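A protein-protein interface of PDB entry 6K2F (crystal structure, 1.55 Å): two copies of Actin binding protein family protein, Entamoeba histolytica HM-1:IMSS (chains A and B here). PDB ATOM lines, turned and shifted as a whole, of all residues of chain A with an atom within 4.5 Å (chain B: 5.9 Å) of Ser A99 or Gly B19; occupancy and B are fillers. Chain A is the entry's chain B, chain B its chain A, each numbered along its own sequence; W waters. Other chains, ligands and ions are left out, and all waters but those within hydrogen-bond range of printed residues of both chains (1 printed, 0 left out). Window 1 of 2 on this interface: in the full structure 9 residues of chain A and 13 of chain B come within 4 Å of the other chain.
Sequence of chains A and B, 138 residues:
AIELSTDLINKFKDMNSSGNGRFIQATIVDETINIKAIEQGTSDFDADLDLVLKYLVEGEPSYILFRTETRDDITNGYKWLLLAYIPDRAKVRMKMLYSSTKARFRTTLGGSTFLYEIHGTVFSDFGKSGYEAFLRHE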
ATOM      1  N   ILE A  86       1.779  -0.659  11.601  1.00  0.00           N
ATOM      2  CA  ILE A  86       3.245  -0.830  11.764  1.00  0.00           C
ATOM      3  C   ILE A  86       3.800  -1.097  10.374  1.00  0.00           C
ATOM      4  O   ILE A  86       3.988  -2.241   9.961  1.00  0.00           O
ATOM      5  CB  ILE A  86       3.583  -1.922  12.790  1.00  0.00           C
ATOM      6  CG1 ILE A  86       2.870  -1.677  14.125  1.00  0.00           C
ATOM      7  CG2 ILE A  86       5.080  -2.032  12.969  1.00  0.00           C
ATOM      8  CD1 ILE A  86       3.075  -2.731  15.177  1.00  0.00           C
ATOM      9  N   LYS A  95       9.560  -0.431  14.673  1.00  0.00           N
ATOM     10  CA  LYS A  95       8.672  -1.609  14.461  1.00  0.00           C
ATOM     11  C   LYS A  95       8.717  -2.500  15.707  1.00  0.00           C
ATOM     12  O   LYS A  95       7.635  -2.951  16.165  1.00  0.00           O
ATOM     13  CB  LYS A  95       9.091  -2.359  13.205  1.00  0.00           C
ATOM     14  CG  LYS A  95       8.841  -1.551  11.929  1.00  0.00           C
ATOM     15  CD  LYS A  95       9.016  -2.338  10.656  1.00  0.00           C
ATOM     16  CE  LYS A  95      10.444  -2.762  10.446  1.00  0.00           C
ATOM     17  NZ  LYS A  95      10.647  -3.381   9.115  1.00  0.00           N
ATOM     18  N   MET A  96       9.901  -2.676  16.284  1.00  0.00           N
ATOM     19  CA  MET A  96      10.082  -3.506  17.496  1.00  0.00           C
ATOM     20  C   MET A  96       9.361  -2.848  18.669  1.00  0.00           C
ATOM     21  O   MET A  96       8.640  -3.530  19.404  1.00  0.00           O
ATOM     22  CB  MET A  96      11.560  -3.695  17.838  1.00  0.00           C
ATOM     23  CG  MET A  96      11.753  -4.290  19.201  1.00  0.00           C
ATOM     24  SD  MET A  96      11.189  -6.023  19.254  1.00  0.00           S
ATOM     25  CE  MET A  96      12.591  -6.849  18.505  1.00  0.00           C
ATOM     26  N   LEU A  97       9.513  -1.534  18.823  1.00  0.00           N
ATOM     27  CA  LEU A  97       8.869  -0.787  19.925  1.00  0.00           C
ATOM     28  C   LEU A  97       7.349  -0.946  19.830  1.00  0.00           C
ATOM     29  O   LEU A  97       6.689  -1.283  20.834  1.00  0.00           O
ATOM     30  CB  LEU A  97       9.268   0.684  19.795  1.00  0.00           C
ATOM     31  CG  LEU A  97       8.893   1.557  20.982  1.00  0.00           C
ATOM     32  CD1 LEU A  97       9.609   1.100  22.241  1.00  0.00           C
ATOM     33  CD2 LEU A  97       9.202   3.014  20.666  1.00  0.00           C
ATOM     34  N   TYR A  98       6.771  -0.730  18.652  1.00  0.00           N
ATOM     35  CA  TYR A  98       5.307  -0.777  18.493  1.00  0.00           C
ATOM     36  C   TYR A  98       4.807  -2.219  18.591  1.00  0.00           C
ATOM     37  O   TYR A  98       3.751  -2.446  19.189  1.00  0.00           O
ATOM     38  CB  TYR A  98       4.867  -0.084  17.214  1.00  0.00           C
ATOM     39  CG  TYR A  98       4.754   1.400  17.385  1.00  0.00           C
ATOM     40  CD1 TYR A  98       5.870   2.205  17.329  1.00  0.00           C
ATOM     41  CD2 TYR A  98       3.545   1.985  17.672  1.00  0.00           C
ATOM     42  CE1 TYR A  98       5.775   3.581  17.515  1.00  0.00           C
ATOM     43  CE2 TYR A  98       3.436   3.349  17.878  1.00  0.00           C
ATOM     44  CZ  TYR A  98       4.549   4.149  17.792  1.00  0.00           C
ATOM     45  OH  TYR A  98       4.504   5.504  18.001  1.00  0.00           O
ATOM     46  N   SER A  99       5.547  -3.177  18.062  1.00  0.00           N
ATOM     47  CA  SER A  99       5.135  -4.602  18.106  1.00  0.00           C
ATOM     48  C   SER A  99       5.121  -5.080  19.563  1.00  0.00           C
ATOM     49  O   SER A  99       4.082  -5.649  20.021  1.00  0.00           O
ATOM     50  CB  SER A  99       6.013  -5.452  17.229  1.00  0.00           C
ATOM     51  OG  SER A  99       5.863  -5.033  15.864  1.00  0.00           O
ATOM     52  N   SER A 100       6.220  -4.833  20.273  1.00  0.00           N
ATOM     53  CA  SER A 100       6.461  -5.365  21.633  1.00  0.00           C
ATOM     54  C   SER A 100       5.524  -4.698  22.642  1.00  0.00           C
ATOM     55  O   SER A 100       5.247  -5.293  23.693  1.00  0.00           O
ATOM     56  CB  SER A 100       7.902  -5.241  22.017  1.00  0.00           C
ATOM     57  OG  SER A 100       8.298  -3.887  22.104  1.00  0.00           O
ATOM     58  N   THR A 101       5.050  -3.489  22.358  1.00  0.00           N
ATOM     59  CA  THR A 101       4.231  -2.692  23.304  1.00  0.00           C
ATOM     60  C   THR A 101       2.738  -3.032  23.174  1.00  0.00           C
ATOM     61  O   THR A 101       1.944  -2.609  24.030  1.00  0.00           O
ATOM     62  CB  THR A 101       4.573  -1.219  23.104  1.00  0.00           C
ATOM     63  OG1 THR A 101       5.959  -1.058  23.411  1.00  0.00           O
ATOM     64  CG2 THR A 101       3.731  -0.305  23.972  1.00  0.00           C
ATOM     65  N   LYS A 102       2.332  -3.776  22.151  1.00  0.00           N
ATOM     66  CA  LYS A 102       0.879  -4.035  21.904  1.00  0.00           C
ATOM     67  C   LYS A 102       0.191  -4.555  23.165  1.00  0.00           C
ATOM     68  O   LYS A 102      -0.949  -4.142  23.452  1.00  0.00           O
ATOM     69  CB  LYS A 102       0.695  -5.056  20.780  1.00  0.00           C
ATOM     70  CG  LYS A 102       0.762  -4.515  19.365  1.00  0.00           C
ATOM     71  CD  LYS A 102       0.772  -5.720  18.431  1.00  0.00           C
ATOM     72  CE  LYS A 102       0.924  -5.493  16.956  1.00  0.00           C
ATOM     73  NZ  LYS A 102       1.004  -6.831  16.317  1.00  0.00           N
ATOM     74  N   ASP B  14      14.468 -10.252   9.795  1.00  0.00           N
ATOM     75  CA  ASP B  14      13.491  -9.141   9.784  1.00  0.00           C
ATOM     76  C   ASP B  14      12.472  -9.347  10.910  1.00  0.00           C
ATOM     77  O   ASP B  14      12.265  -8.411  11.710  1.00  0.00           O
ATOM     78  CB  ASP B  14      12.815  -8.988   8.426  1.00  0.00           C
ATOM     79  CG  ASP B  14      11.968  -7.729   8.377  1.00  0.00           C
ATOM     80  OD1 ASP B  14      12.465  -6.691   8.848  1.00  0.00           O
ATOM     81  OD2 ASP B  14      10.810  -7.809   7.921  1.00  0.00           O
ATOM     82  N   MET B  15      11.872 -10.531  11.001  1.00  0.00           N
ATOM     83  CA  MET B  15      10.862 -10.815  12.048  1.00  0.00           C
ATOM     84  C   MET B  15      11.516 -10.782  13.431  1.00  0.00           C
ATOM     85  O   MET B  15      10.904 -10.238  14.376  1.00  0.00           O
ATOM     86  CB  MET B  15      10.197 -12.168  11.814  1.00  0.00           C
ATOM     87  CG  MET B  15       8.964 -12.340  12.669  1.00  0.00           C
ATOM     88  SD  MET B  15       8.022 -13.851  12.309  1.00  0.00           S
ATOM     89  CE  MET B  15       7.476 -13.527  10.635  1.00  0.00           C
ATOM     90  N   ASN B  16      12.754 -11.262  13.544  1.00  0.00           N
ATOM     91  CA  ASN B  16      13.515 -11.280  14.815  1.00  0.00           C
ATOM     92  C   ASN B  16      13.777  -9.842  15.275  1.00  0.00           C
ATOM     93  O   ASN B  16      13.568  -9.534  16.453  1.00  0.00           O
ATOM     94  CB  ASN B  16      14.829 -12.045  14.670  1.00  0.00           C
ATOM     95  CG  ASN B  16      15.578 -12.175  15.975  1.00  0.00           C
ATOM     96  OD1 ASN B  16      15.024 -12.643  16.969  1.00  0.00           O
ATOM     97  ND2 ASN B  16      16.823 -11.729  16.000  1.00  0.00           N
ATOM     98  N   SER B  17      14.253  -8.979  14.386  1.00  0.00           N
ATOM     99  CA  SER B  17      14.662  -7.606  14.752  1.00  0.00           C
ATOM    100  C   SER B  17      13.438  -6.696  14.922  1.00  0.00           C
ATOM    101  O   SER B  17      13.562  -5.715  15.674  1.00  0.00           O
ATOM    102  CB  SER B  17      15.639  -7.068  13.738  1.00  0.00           C
ATOM    103  OG  SER B  17      15.002  -6.888  12.480  1.00  0.00           O
ATOM    104  N   SER B  18      12.337  -6.944  14.197  1.00  0.00           N
ATOM    105  CA  SER B  18      11.163  -6.026  14.138  1.00  0.00           C
ATOM    106  C   SER B  18      10.059  -6.531  15.060  1.00  0.00           C
ATOM    107  O   SER B  18       9.161  -5.750  15.359  1.00  0.00           O
ATOM    108  CB  SER B  18      10.674  -5.878  12.727  1.00  0.00           C
ATOM    109  OG  SER B  18      11.745  -5.540  11.854  1.00  0.00           O
ATOM    110  N   GLY B  19      10.102  -7.807  15.466  1.00  0.00           N
ATOM    111  CA  GLY B  19       9.104  -8.393  16.377  1.00  0.00           C
ATOM    112  C   GLY B  19       7.706  -8.421  15.782  1.00  0.00           C
ATOM    113  O   GLY B  19       6.760  -8.607  16.552  1.00  0.00           O
ATOM    114  N   ASN B  20       7.563  -8.293  14.452  1.00  0.00           N
ATOM    115  CA  ASN B  20       6.298  -7.868  13.787  1.00  0.00           C
ATOM    116  C   ASN B  20       5.625  -9.050  13.081  1.00  0.00           C
ATOM    117  O   ASN B  20       4.898  -8.845  12.106  1.00  0.00           O
ATOM    118  CB  ASN B  20       6.498  -6.711  12.804  1.00  0.00           C
ATOM    119  CG  ASN B  20       7.486  -7.012  11.695  1.00  0.00           C
ATOM    120  OD1 ASN B  20       8.134  -8.063  11.687  1.00  0.00           O
ATOM    121  ND2 ASN B  20       7.617  -6.081  10.766  1.00  0.00           N
ATOM    122  N   GLY B  21       5.786 -10.233  13.628  1.00  0.00           N
ATOM    123  CA  GLY B  21       5.115 -11.465  13.180  1.00  0.00           C
ATOM    124  C   GLY B  21       5.359 -12.521  14.224  1.00  0.00           C
ATOM    125  O   GLY B  21       6.177 -12.264  15.133  1.00  0.00           O
ATOM    126  N   GLN B  40       1.408 -13.741  10.920  1.00  0.00           N
ATOM    127  CA  GLN B  40       1.554 -12.461  11.652  1.00  0.00           C
ATOM    128  C   GLN B  40       1.286 -12.728  13.129  1.00  0.00           C
ATOM    129  O   GLN B  40       1.984 -12.145  13.968  1.00  0.00           O
ATOM    130  CB  GLN B  40       0.582 -11.432  11.088  1.00  0.00           C
ATOM    131  CG  GLN B  40       0.566 -10.131  11.867  1.00  0.00           C
ATOM    132  CD  GLN B  40       1.909  -9.454  11.806  1.00  0.00           C
ATOM    133  OE1 GLN B  40       2.490  -9.276  10.736  1.00  0.00           O
ATOM    134  NE2 GLN B  40       2.397  -9.051  12.967  1.00  0.00           N
ATOM    135  N   SER B  43      -0.233 -10.332  19.783  1.00  0.00           N
ATOM    136  CA  SER B  43       0.621 -10.075  20.959  1.00  0.00           C
ATOM    137  C   SER B  43       0.435 -11.199  21.997  1.00  0.00           C
ATOM    138  O   SER B  43       1.053 -11.081  23.067  1.00  0.00           O
ATOM    139  CB  SER B  43       0.303  -8.745  21.536  1.00  0.00           C
ATOM    140  OG  SER B  43      -1.016  -8.742  22.037  1.00  0.00           O
ATOM    141  N   ARG B  67       8.234 -17.471  17.360  1.00  0.00           N
ATOM    142  CA  ARG B  67       8.840 -16.400  18.185  1.00  0.00           C
ATOM    143  C   ARG B  67       8.228 -16.407  19.589  1.00  0.00           C
ATOM    144  O   ARG B  67       7.005 -16.429  19.705  1.00  0.00           O
ATOM    145  CB  ARG B  67       8.625 -15.048  17.512  1.00  0.00           C
ATOM    146  CG  ARG B  67       9.386 -13.918  18.187  1.00  0.00           C
ATOM    147  CD  ARG B  67       9.163 -12.567  17.532  1.00  0.00           C
ATOM    148  NE  ARG B  67       7.749 -12.242  17.421  1.00  0.00           N
ATOM    149  CZ  ARG B  67       6.957 -11.846  18.409  1.00  0.00           C
ATOM    150  NH1 ARG B  67       7.426 -11.709  19.638  1.00  0.00           N
ATOM    151  NH2 ARG B  67       5.686 -11.574  18.170  1.00  0.00           N
ATOM    152  N   TYR B  78      14.611 -11.641  19.592  1.00  0.00           N
ATOM    153  CA  TYR B  78      13.813 -12.536  20.458  1.00  0.00           C
ATOM    154  C   TYR B  78      14.460 -13.920  20.520  1.00  0.00           C
ATOM    155  O   TYR B  78      15.207 -14.325  19.610  1.00  0.00           O
ATOM    156  CB  TYR B  78      12.403 -12.648  19.895  1.00  0.00           C
ATOM    157  CG  TYR B  78      11.485 -11.505  20.237  1.00  0.00           C
ATOM    158  CD1 TYR B  78      10.799 -11.510  21.440  1.00  0.00           C
ATOM    159  CD2 TYR B  78      11.266 -10.443  19.372  1.00  0.00           C
ATOM    160  CE1 TYR B  78       9.899 -10.516  21.769  1.00  0.00           C
ATOM    161  CE2 TYR B  78      10.359  -9.440  19.689  1.00  0.00           C
ATOM    162  CZ  TYR B  78       9.684  -9.467  20.899  1.00  0.00           C
ATOM    163  OH  TYR B  78       8.774  -8.501  21.274  1.00  0.00           O
HETATM  164  O   HOH W   1       6.643  -8.059  19.332  1.00  0.00           O
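The backbone carbonyl oxygen (O) of Asp B14 lies within hydrogen-bond range of the side-chain hydroxyl (OG) of Ser B17, at 3.2 Å.
The side-chain hydroxyl of Ser B18 is in hydrogen-bond range of the backbone carbonyl oxygen of Asp B14, 2.9 Å away.
N of Tyr B78 is in hydrogen-bond range of OD1 of Asn B16, 2.8 Å away.
The backbone carbonyl oxygen of Asn B20 lies within hydrogen-bond range of the side-chain amide nitrogen of Gln B40, 2.7 Å away.
The side-chain hydroxyl of Ser A99 lies within hydrogen-bond range of the backbone carbonyl oxygen of Lys A95, 2.8 Å away.
O of Leu A97 sits at hydrogen-bond distance from OG of Ser A100, at 3.3 Å.
CD of Lys A95 touches ND2 of Asn B20, 3.997 Å away.
Asn B16 touches Met A96 (O to CE, 3.5 Å).
CE of Met A96 touches O of Ser B17, 3.2 Å away.
SD of Met A96 touches CE2 of Tyr B78, 3.5 Å away.
Gly B19 touches Ser A99 (O to CB, 3.3 Å).
Ser A99 touches Asn B20 (OG to CA, 3.5 Å).
Tyr B78 touches Ser A100 (OH to CB, 3.5 Å).
Lys A102 touches Ser B43 (CB to CB, 3.8 Å).
No position is printed for both chains.
Of the 12 pairs that touch across the chains among the printed residues, none has its exchanged pair printed and touching as well.
OD1 of Asp B14 is in salt-bridge range of NZ of Lys A95, at 3.8 Å.
O of Ser B18 sits close to N of Met A96, at 3.3 Å.
The backbone carbonyl oxygen (O) of Ser B18 sits at hydrogen-bond distance from the side-chain hydroxyl (OG) of Ser A99 (3.4 Å).
The backbone carbonyl oxygen (O) of Lys A95 lies close to the backbone carbonyl oxygen (O) of Ser B18 (3.3 Å).
Water W1 lies within hydrogen-bond range of O of Gly B19, OH of Tyr B78 and N of Ser A100.
Ser A99 touches just these residues of chain B: Ser B18 (3.4 Å), Gly B19 (3.3 Å) and Asn B20 (3.5 Å).
Of chain A, only Ser A99 comes within 4 Å of Gly B19.
Of the printed residues of chain B, Met A96 touches Asn B16 (3.5 Å), Ser B17 (3.2 Å), Ser B18 (3.2 Å) and Tyr B78 (3.5 Å).
Of the printed residues of chain B, Lys A102 touches Ser B43 (3.8 Å).
Of the printed residues of chain B, Ser A100 touches Tyr B78.
Of the printed residues of chain A, Asn B16 touches Met A96.
Of the printed residues of chain A, Ser B43 touches Lys A102.
Gly B21 touches none of the printed residues of chain A.
The nearest residue of chain A that does not touch Gly B19 is Met A96 (4.04 Å).
Of the 12 printed residues of chain B, 8 touch a printed residue of chain A.
Of the 9 printed residues of chain A, 5 touch a printed residue of chain B.
Among the printed residues, Asp or Glu carboxylates within 4 Å of a Lys or Arg side-chain nitrogen of the other chain: Lys A95 with Asp B14.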
